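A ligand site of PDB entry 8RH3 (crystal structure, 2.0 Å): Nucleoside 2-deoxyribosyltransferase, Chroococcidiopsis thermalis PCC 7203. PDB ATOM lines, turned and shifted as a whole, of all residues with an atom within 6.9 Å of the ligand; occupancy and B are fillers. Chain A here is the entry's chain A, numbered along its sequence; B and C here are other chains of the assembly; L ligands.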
ATOM      1  N   TYR A   8     -21.168  20.104  -8.745  1.00  0.00           N
ATOM      2  CA  TYR A   8     -20.540  18.852  -8.306  1.00  0.00           C
ATOM      3  C   TYR A   8     -19.043  18.897  -8.626  1.00  0.00           C
ATOM      4  O   TYR A   8     -18.666  19.023  -9.798  1.00  0.00           O
ATOM      5  CB  TYR A   8     -21.194  17.663  -8.999  1.00  0.00           C
ATOM      6  CG  TYR A   8     -20.702  16.335  -8.525  1.00  0.00           C
ATOM      7  CD1 TYR A   8     -21.274  15.726  -7.413  1.00  0.00           C
ATOM      8  CD2 TYR A   8     -19.661  15.683  -9.172  1.00  0.00           C
ATOM      9  CE1 TYR A   8     -20.809  14.482  -6.974  1.00  0.00           C
ATOM     10  CE2 TYR A   8     -19.185  14.448  -8.732  1.00  0.00           C
ATOM     11  CZ  TYR A   8     -19.772  13.857  -7.644  1.00  0.00           C
ATOM     12  OH  TYR A   8     -19.337  12.625  -7.206  1.00  0.00           O
ATOM     13  N   LEU A   9     -18.197  18.831  -7.595  1.00  0.00           N
ATOM     14  CA  LEU A   9     -16.740  19.017  -7.742  1.00  0.00           C
ATOM     15  C   LEU A   9     -16.090  17.646  -7.857  1.00  0.00           C
ATOM     16  O   LEU A   9     -15.706  17.031  -6.856  1.00  0.00           O
ATOM     17  CB  LEU A   9     -16.181  19.808  -6.564  1.00  0.00           C
ATOM     18  CG  LEU A   9     -14.658  19.972  -6.455  1.00  0.00           C
ATOM     19  CD1 LEU A   9     -14.080  20.508  -7.757  1.00  0.00           C
ATOM     20  CD2 LEU A   9     -14.312  20.856  -5.275  1.00  0.00           C
ATOM     21  N   ALA A  10     -15.956  17.156  -9.086  1.00  0.00           N
ATOM     22  CA  ALA A  10     -15.369  15.852  -9.319  1.00  0.00           C
ATOM     23  C   ALA A  10     -13.845  15.973  -9.433  1.00  0.00           C
ATOM     24  O   ALA A  10     -13.339  16.818 -10.181  1.00  0.00           O
ATOM     25  CB  ALA A  10     -15.944  15.233 -10.593  1.00  0.00           C
ATOM     26  N   SER A  11     -13.115  15.116  -8.710  1.00  0.00           N
ATOM     27  CA  SER A  11     -11.659  15.196  -8.697  1.00  0.00           C
ATOM     28  C   SER A  11     -11.091  13.867  -8.195  1.00  0.00           C
ATOM     29  O   SER A  11     -11.817  13.064  -7.595  1.00  0.00           O
ATOM     30  CB  SER A  11     -11.184  16.361  -7.809  1.00  0.00           C
ATOM     31  OG  SER A  11     -11.002  15.932  -6.466  1.00  0.00           O
ATOM     32  N   PRO A  12      -9.806  13.603  -8.449  1.00  0.00           N
ATOM     33  CA  PRO A  12      -9.117  12.492  -7.780  1.00  0.00           C
ATOM     34  C   PRO A  12      -8.516  12.859  -6.424  1.00  0.00           C
ATOM     35  O   PRO A  12      -7.988  11.972  -5.748  1.00  0.00           O
ATOM     36  CB  PRO A  12      -8.006  12.108  -8.776  1.00  0.00           C
ATOM     37  CG  PRO A  12      -7.796  13.321  -9.641  1.00  0.00           C
ATOM     38  CD  PRO A  12      -8.933  14.291  -9.414  1.00  0.00           C
ATOM     39  N   PHE A  15      -8.240  10.918  -2.920  1.00  0.00           N
ATOM     40  CA  PHE A  15      -7.559   9.628  -2.807  1.00  0.00           C
ATOM     41  C   PHE A  15      -6.234   9.750  -2.052  1.00  0.00           C
ATOM     42  O   PHE A  15      -5.782   8.757  -1.465  1.00  0.00           O
ATOM     43  CB  PHE A  15      -7.307   9.060  -4.227  1.00  0.00           C
ATOM     44  CG  PHE A  15      -8.560   8.575  -4.919  1.00  0.00           C
ATOM     45  CD1 PHE A  15      -9.424   7.680  -4.299  1.00  0.00           C
ATOM     46  CD2 PHE A  15      -8.871   9.023  -6.191  1.00  0.00           C
ATOM     47  CE1 PHE A  15     -10.568   7.230  -4.948  1.00  0.00           C
ATOM     48  CE2 PHE A  15     -10.006   8.585  -6.849  1.00  0.00           C
ATOM     49  CZ  PHE A  15     -10.878   7.687  -6.218  1.00  0.00           C
ATOM     50  N   GLU A  40     -18.788  18.459  -2.878  1.00  0.00           N
ATOM     51  CA  GLU A  40     -17.523  17.754  -2.958  1.00  0.00           C
ATOM     52  C   GLU A  40     -17.714  16.309  -2.500  1.00  0.00           C
ATOM     53  O   GLU A  40     -17.913  16.082  -1.294  1.00  0.00           O
ATOM     54  CB  GLU A  40     -16.474  18.454  -2.105  1.00  0.00           C
ATOM     55  CG  GLU A  40     -15.011  18.086  -2.389  1.00  0.00           C
ATOM     56  CD  GLU A  40     -14.678  16.660  -1.946  1.00  0.00           C
ATOM     57  OE1 GLU A  40     -14.579  16.423  -0.723  1.00  0.00           O
ATOM     58  OE2 GLU A  40     -14.563  15.776  -2.829  1.00  0.00           O
ATOM     59  N   PRO A  41     -17.623  15.316  -3.399  1.00  0.00           N
ATOM     60  CA  PRO A  41     -18.153  13.985  -3.068  1.00  0.00           C
ATOM     61  C   PRO A  41     -17.365  13.213  -2.026  1.00  0.00           C
ATOM     62  O   PRO A  41     -17.936  12.332  -1.360  1.00  0.00           O
ATOM     63  CB  PRO A  41     -18.142  13.264  -4.414  1.00  0.00           C
ATOM     64  CG  PRO A  41     -17.089  13.974  -5.226  1.00  0.00           C
ATOM     65  CD  PRO A  41     -17.086  15.393  -4.761  1.00  0.00           C
ATOM     66  N   PHE A  42     -16.057  13.470  -1.873  1.00  0.00           N
ATOM     67  CA  PHE A  42     -15.292  12.717  -0.895  1.00  0.00           C
ATOM     68  C   PHE A  42     -15.790  13.041   0.510  1.00  0.00           C
ATOM     69  O   PHE A  42     -16.061  12.138   1.316  1.00  0.00           O
ATOM     70  CB  PHE A  42     -13.795  13.007  -1.051  1.00  0.00           C
ATOM     71  CG  PHE A  42     -13.165  12.303  -2.230  1.00  0.00           C
ATOM     72  CD1 PHE A  42     -12.983  10.924  -2.232  1.00  0.00           C
ATOM     73  CD2 PHE A  42     -12.790  13.010  -3.363  1.00  0.00           C
ATOM     74  CE1 PHE A  42     -12.419  10.273  -3.330  1.00  0.00           C
ATOM     75  CE2 PHE A  42     -12.226  12.369  -4.459  1.00  0.00           C
ATOM     76  CZ  PHE A  42     -12.039  11.004  -4.436  1.00  0.00           C
ATOM     77  N   ASN A  45     -20.026  12.399   0.744  1.00  0.00           N
ATOM     78  CA  ASN A  45     -20.484  11.026   0.797  1.00  0.00           C
ATOM     79  C   ASN A  45     -19.542  10.104   1.568  1.00  0.00           C
ATOM     80  O   ASN A  45     -19.695   8.881   1.513  1.00  0.00           O
ATOM     81  CB  ASN A  45     -20.739  10.502  -0.614  1.00  0.00           C
ATOM     82  CG  ASN A  45     -21.849  11.266  -1.305  1.00  0.00           C
ATOM     83  OD1 ASN A  45     -22.873  11.570  -0.675  1.00  0.00           O
ATOM     84  ND2 ASN A  45     -21.650  11.624  -2.568  1.00  0.00           N
ATOM     85  N   GLN A  47     -16.109   9.141   1.731  1.00  0.00           N
ATOM     86  CA  GLN A  47     -15.195   8.187   1.106  1.00  0.00           C
ATOM     87  C   GLN A  47     -13.802   8.569   1.617  1.00  0.00           C
ATOM     88  O   GLN A  47     -13.096   9.402   1.029  1.00  0.00           O
ATOM     89  CB  GLN A  47     -15.331   8.180  -0.433  1.00  0.00           C
ATOM     90  CG  GLN A  47     -15.092   6.782  -1.020  1.00  0.00           C
ATOM     91  CD  GLN A  47     -14.525   6.749  -2.440  1.00  0.00           C
ATOM     92  OE1 GLN A  47     -14.807   7.624  -3.270  1.00  0.00           O
ATOM     93  NE2 GLN A  47     -13.744   5.700  -2.730  1.00  0.00           N
ATOM     94  N   VAL A  59     -21.641   4.399  -1.779  1.00  0.00           N
ATOM     95  CA  VAL A  59     -20.798   5.493  -2.286  1.00  0.00           C
ATOM     96  C   VAL A  59     -21.095   5.737  -3.766  1.00  0.00           C
ATOM     97  O   VAL A  59     -21.355   6.864  -4.192  1.00  0.00           O
ATOM     98  CB  VAL A  59     -19.310   5.205  -2.035  1.00  0.00           C
ATOM     99  CG1 VAL A  59     -18.456   6.402  -2.430  1.00  0.00           C
ATOM    100  CG2 VAL A  59     -19.077   4.917  -0.576  1.00  0.00           C
ATOM    101  N   ALA A  60     -21.076   4.666  -4.559  1.00  0.00           N
ATOM    102  CA  ALA A  60     -21.365   4.761  -5.988  1.00  0.00           C
ATOM    103  C   ALA A  60     -22.701   5.459  -6.245  1.00  0.00           C
ATOM    104  O   ALA A  60     -22.764   6.445  -6.989  1.00  0.00           O
ATOM    105  CB  ALA A  60     -21.363   3.361  -6.596  1.00  0.00           C
ATOM    106  N   ASP A  63     -22.560   9.267  -5.129  1.00  0.00           N
ATOM    107  CA  ASP A  63     -21.922  10.109  -6.155  1.00  0.00           C
ATOM    108  C   ASP A  63     -22.823  10.260  -7.374  1.00  0.00           C
ATOM    109  O   ASP A  63     -22.983  11.352  -7.922  1.00  0.00           O
ATOM    110  CB  ASP A  63     -20.554   9.547  -6.625  1.00  0.00           C
ATOM    111  CG  ASP A  63     -19.434   9.676  -5.598  1.00  0.00           C
ATOM    112  OD1 ASP A  63     -19.691  10.216  -4.492  1.00  0.00           O
ATOM    113  OD2 ASP A  63     -18.266   9.255  -5.939  1.00  0.00           O
ATOM    114  N   LEU A  64     -23.392   9.134  -7.822  1.00  0.00           N
ATOM    115  CA  LEU A  64     -24.238   9.141  -9.018  1.00  0.00           C
ATOM    116  C   LEU A  64     -25.461  10.017  -8.813  1.00  0.00           C
ATOM    117  O   LEU A  64     -25.822  10.816  -9.692  1.00  0.00           O
ATOM    118  CB  LEU A  64     -24.644   7.706  -9.351  1.00  0.00           C
ATOM    119  CG  LEU A  64     -25.729   7.489 -10.409  1.00  0.00           C
ATOM    120  CD1 LEU A  64     -25.449   6.229 -11.165  1.00  0.00           C
ATOM    121  CD2 LEU A  64     -27.101   7.352  -9.736  1.00  0.00           C
ATOM    122  N   ASP A  83      -8.662  11.053 -14.157  1.00  0.00           N
ATOM    123  CA  ASP A  83      -9.190   9.994 -13.306  1.00  0.00           C
ATOM    124  C   ASP A  83     -10.429   9.342 -13.922  1.00  0.00           C
ATOM    125  O   ASP A  83     -11.314  10.035 -14.431  1.00  0.00           O
ATOM    126  CB  ASP A  83      -9.531  10.569 -11.932  1.00  0.00           C
ATOM    127  CG  ASP A  83     -10.017   9.517 -10.961  1.00  0.00           C
ATOM    128  OD1 ASP A  83      -9.181   8.880 -10.269  1.00  0.00           O
ATOM    129  OD2 ASP A  83     -11.253   9.339 -10.883  1.00  0.00           O
ATOM    130  N   GLU A  84     -10.487   8.006 -13.847  1.00  0.00           N
ATOM    131  CA  GLU A  84     -11.561   7.274 -14.504  1.00  0.00           C
ATOM    132  C   GLU A  84     -12.923   7.520 -13.829  1.00  0.00           C
ATOM    133  O   GLU A  84     -13.958   7.517 -14.498  1.00  0.00           O
ATOM    134  CB  GLU A  84     -11.218   5.770 -14.570  1.00  0.00           C
ATOM    135  CG  GLU A  84     -11.081   5.016 -13.247  1.00  0.00           C
ATOM    136  CD  GLU A  84      -9.685   5.114 -12.606  1.00  0.00           C
ATOM    137  OE1 GLU A  84      -8.861   5.954 -13.055  1.00  0.00           O
ATOM    138  OE2 GLU A  84      -9.408   4.356 -11.636  1.00  0.00           O
ATOM    139  N   GLY A  85     -12.930   7.753 -12.518  1.00  0.00           N
ATOM    140  CA  GLY A  85     -14.189   8.044 -11.838  1.00  0.00           C
ATOM    141  C   GLY A  85     -14.729   9.422 -12.184  1.00  0.00           C
ATOM    142  O   GLY A  85     -15.915   9.586 -12.451  1.00  0.00           O
ATOM    143  N   VAL A  86     -13.849  10.423 -12.207  1.00  0.00           N
ATOM    144  CA  VAL A  86     -14.205  11.734 -12.721  1.00  0.00           C
ATOM    145  C   VAL A  86     -14.755  11.640 -14.135  1.00  0.00           C
ATOM    146  O   VAL A  86     -15.733  12.324 -14.483  1.00  0.00           O
ATOM    147  CB  VAL A  86     -12.984  12.662 -12.657  1.00  0.00           C
ATOM    148  CG1 VAL A  86     -13.297  13.992 -13.321  1.00  0.00           C
ATOM    149  CG2 VAL A  86     -12.581  12.848 -11.211  1.00  0.00           C
ATOM    150  N   MET A  87     -14.175  10.781 -14.969  1.00  0.00           N
ATOM    151  CA  MET A  87     -14.581  10.740 -16.373  1.00  0.00           C
ATOM    152  C   MET A  87     -15.950  10.104 -16.528  1.00  0.00           C
ATOM    153  O   MET A  87     -16.722  10.461 -17.427  1.00  0.00           O
ATOM    154  CB  MET A  87     -13.576   9.948 -17.223  1.00  0.00           C
ATOM    155  CG  MET A  87     -12.212  10.572 -17.323  1.00  0.00           C
ATOM    156  SD  MET A  87     -12.199  11.983 -18.382  1.00  0.00           S
ATOM    157  CE  MET A  87     -12.368  13.297 -17.124  1.00  0.00           C
ATOM    158  N   GLU A  89     -18.366  10.235 -14.262  1.00  0.00           N
ATOM    159  CA  GLU A  89     -19.169  11.368 -13.817  1.00  0.00           C
ATOM    160  C   GLU A  89     -19.304  12.440 -14.902  1.00  0.00           C
ATOM    161  O   GLU A  89     -20.402  12.952 -15.129  1.00  0.00           O
ATOM    162  CB  GLU A  89     -18.551  11.908 -12.531  1.00  0.00           C
ATOM    163  CG  GLU A  89     -18.754  10.929 -11.347  1.00  0.00           C
ATOM    164  CD  GLU A  89     -18.006  11.312 -10.076  1.00  0.00           C
ATOM    165  OE1 GLU A  89     -17.294  12.344 -10.071  1.00  0.00           O
ATOM    166  OE2 GLU A  89     -18.113  10.558  -9.089  1.00  0.00           O
ATOM    167  N   ASP B 112     -10.377   1.449  -5.745  1.00  0.00           N
ATOM    168  CA  ASP B 112     -10.499   2.304  -4.563  1.00  0.00           C
ATOM    169  C   ASP B 112     -11.405   1.674  -3.502  1.00  0.00           C
ATOM    170  O   ASP B 112     -11.792   2.366  -2.550  1.00  0.00           O
ATOM    171  CB  ASP B 112     -11.034   3.699  -4.936  1.00  0.00           C
ATOM    172  CG  ASP B 112     -12.449   3.684  -5.571  1.00  0.00           C
ATOM    173  OD1 ASP B 112     -12.922   2.625  -6.049  1.00  0.00           O
ATOM    174  OD2 ASP B 112     -13.103   4.751  -5.594  1.00  0.00           O
ATOM    175  N   ASN B 119     -12.180   1.199  -9.879  1.00  0.00           N
ATOM    176  CA  ASN B 119     -12.960   2.345  -9.413  1.00  0.00           C
ATOM    177  C   ASN B 119     -14.452   2.064  -9.403  1.00  0.00           C
ATOM    178  O   ASN B 119     -15.011   1.632 -10.416  1.00  0.00           O
ATOM    179  CB  ASN B 119     -12.645   3.579 -10.260  1.00  0.00           C
ATOM    180  CG  ASN B 119     -13.227   4.845  -9.659  1.00  0.00           C
ATOM    181  OD1 ASN B 119     -14.458   5.001  -9.551  1.00  0.00           O
ATOM    182  ND2 ASN B 119     -12.360   5.746  -9.243  1.00  0.00           N
ATOM    183  N   LEU B 120     -15.110   2.282  -8.262  1.00  0.00           N
ATOM    184  CA  LEU B 120     -16.469   1.760  -8.081  1.00  0.00           C
ATOM    185  C   LEU B 120     -17.474   2.470  -8.974  1.00  0.00           C
ATOM    186  O   LEU B 120     -18.537   1.914  -9.288  1.00  0.00           O
ATOM    187  CB  LEU B 120     -16.906   1.888  -6.615  1.00  0.00           C
ATOM    188  CG  LEU B 120     -16.663   3.214  -5.893  1.00  0.00           C
ATOM    189  CD1 LEU B 120     -17.833   4.161  -6.068  1.00  0.00           C
ATOM    190  CD2 LEU B 120     -16.376   2.992  -4.415  1.00  0.00           C
ATOM    191  N   MET B 121     -17.166   3.696  -9.411  1.00  0.00           N
ATOM    192  CA  MET B 121     -18.076   4.427 -10.284  1.00  0.00           C
ATOM    193  C   MET B 121     -18.370   3.664 -11.576  1.00  0.00           C
ATOM    194  O   MET B 121     -19.490   3.727 -12.094  1.00  0.00           O
ATOM    195  CB  MET B 121     -17.485   5.812 -10.558  1.00  0.00           C
ATOM    196  CG  MET B 121     -17.799   6.853  -9.489  1.00  0.00           C
ATOM    197  SD  MET B 121     -19.454   6.659  -8.749  1.00  0.00           S
ATOM    198  CE  MET B 121     -20.406   7.733  -9.803  1.00  0.00           C
ATOM    199  N   ARG C 108      -5.656   4.176  -2.955  1.00  0.00           N
ATOM    200  CA  ARG C 108      -6.065   3.232  -3.982  1.00  0.00           C
ATOM    201  C   ARG C 108      -5.015   2.141  -4.132  1.00  0.00           C
ATOM    202  O   ARG C 108      -3.815   2.376  -3.955  1.00  0.00           O
ATOM    203  CB  ARG C 108      -6.264   3.960  -5.311  1.00  0.00           C
ATOM    204  CG  ARG C 108      -7.558   4.740  -5.384  1.00  0.00           C
ATOM    205  CD  ARG C 108      -7.606   5.509  -6.666  1.00  0.00           C
ATOM    206  NE  ARG C 108      -6.437   6.375  -6.780  1.00  0.00           N
ATOM    207  CZ  ARG C 108      -6.134   7.081  -7.858  1.00  0.00           C
ATOM    208  NH1 ARG C 108      -6.917   7.082  -8.930  1.00  0.00           N
ATOM    209  NH2 ARG C 108      -5.008   7.787  -7.872  1.00  0.00           N
HETATM  210  C1  LIG L   1     -15.033   9.999  -6.892  1.00  0.00           C
HETATM  211  C2  LIG L   1     -16.397   9.756  -6.060  1.00  0.00           C
HETATM  212  C3  LIG L   1     -17.245   8.936  -6.815  1.00  0.00           C
HETATM  213  C4  LIG L   1     -15.246   8.829  -7.733  1.00  0.00           C
HETATM  214  C5  LIG L   1     -13.871   8.235  -7.823  1.00  0.00           C
HETATM  215  O1  LIG L   1     -14.992  11.215  -7.736  1.00  0.00           O
HETATM  216  O2  LIG L   1     -16.251   8.043  -6.994  1.00  0.00           O
HETATM  217  O3  LIG L   1     -13.062   9.180  -8.577  1.00  0.00           O
HETATM  218  F1  LIG L   1     -16.326   8.939  -5.102  1.00  0.00           F
HETATM  219  F2  LIG L   1     -16.991  10.868  -5.691  1.00  0.00           F
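A carbon (C3) of the ligand is covalently linked to the side-chain carboxylate (OD2) of Asp 63 (1.4 Å).
The side-chain carboxylate (OE2) of Glu 89 lies close to an oxygen (O1) of the ligand (3.5 Å).
An oxygen (O3) of the ligand is in hydrogen-bond range of the side-chain carboxylate of Asp 83, 2.9 Å away.
The side-chain carboxylate (OD1) of Asp 83 lies within salt-bridge range of the guanidinium group (NH1) of Arg 108 of chain C (3.2 Å).
The side-chain amide nitrogen (NE2) of Gln 47 is in hydrogen-bond range of the side-chain carboxylate (OD2) of Asp 112 of chain B (3.1 Å).
The side-chain carboxylate (OD2) of Asp 83 sits at hydrogen-bond distance from the backbone NH (N) of Val 86, 3.1 Å away.
The side-chain carboxylate (OD1) of Asp 63 sits at hydrogen-bond distance from the side-chain amide nitrogen (ND2) of Asn 45, at 3.1 Å.
The side-chain carboxylate of Glu 89 lies within hydrogen-bond range of the side-chain hydroxyl of Tyr 8, 3.1 Å away.
OD1 of Asn 119 of chain B sits at hydrogen-bond distance from N of Met 121 of chain B (3.0 Å).
The backbone NH (N) of Gln 47 lies within hydrogen-bond range of the backbone carbonyl oxygen (O) of Phe 42 (3.0 Å).
The side-chain carboxylate (OD2) of Asp 83 is in hydrogen-bond range of the backbone NH (N) of Gly 85, 2.8 Å away.
The side-chain hydroxyl (OH) of Tyr 8 lies close to a fluorine (F2) of the ligand (3.3 Å).
F1 of the ligand lies close to OE1 of Gln 47 (2.7 Å).
O of Ser 11 touches O1 of the ligand (3.7 Å).
CZ of Phe 15 touches C5 of the ligand, at 3.4 Å.
Pro 41 touches the ligand (CB to F2, 2.9 Å).
Gly 85 touches the ligand.
Val 86 touches the ligand (N to O3, 3.9 Å).
Asn 119 of chain B touches the ligand.
Met 121 of chain B touches the ligand (CG to O2, 3.2 Å).
Hydrophobic or aromatic side chains that line the ligand: Phe 15, Pro 41 and Met 121 of chain B.
Within 4 Å of the ligand: Tyr 8, Ser 11, Phe 15, Pro 41, Gln 47, Asp 63, Asp 83, Gly 85, Val 86, Glu 89, Asn 119 of chain B and Met 121 of chain B.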
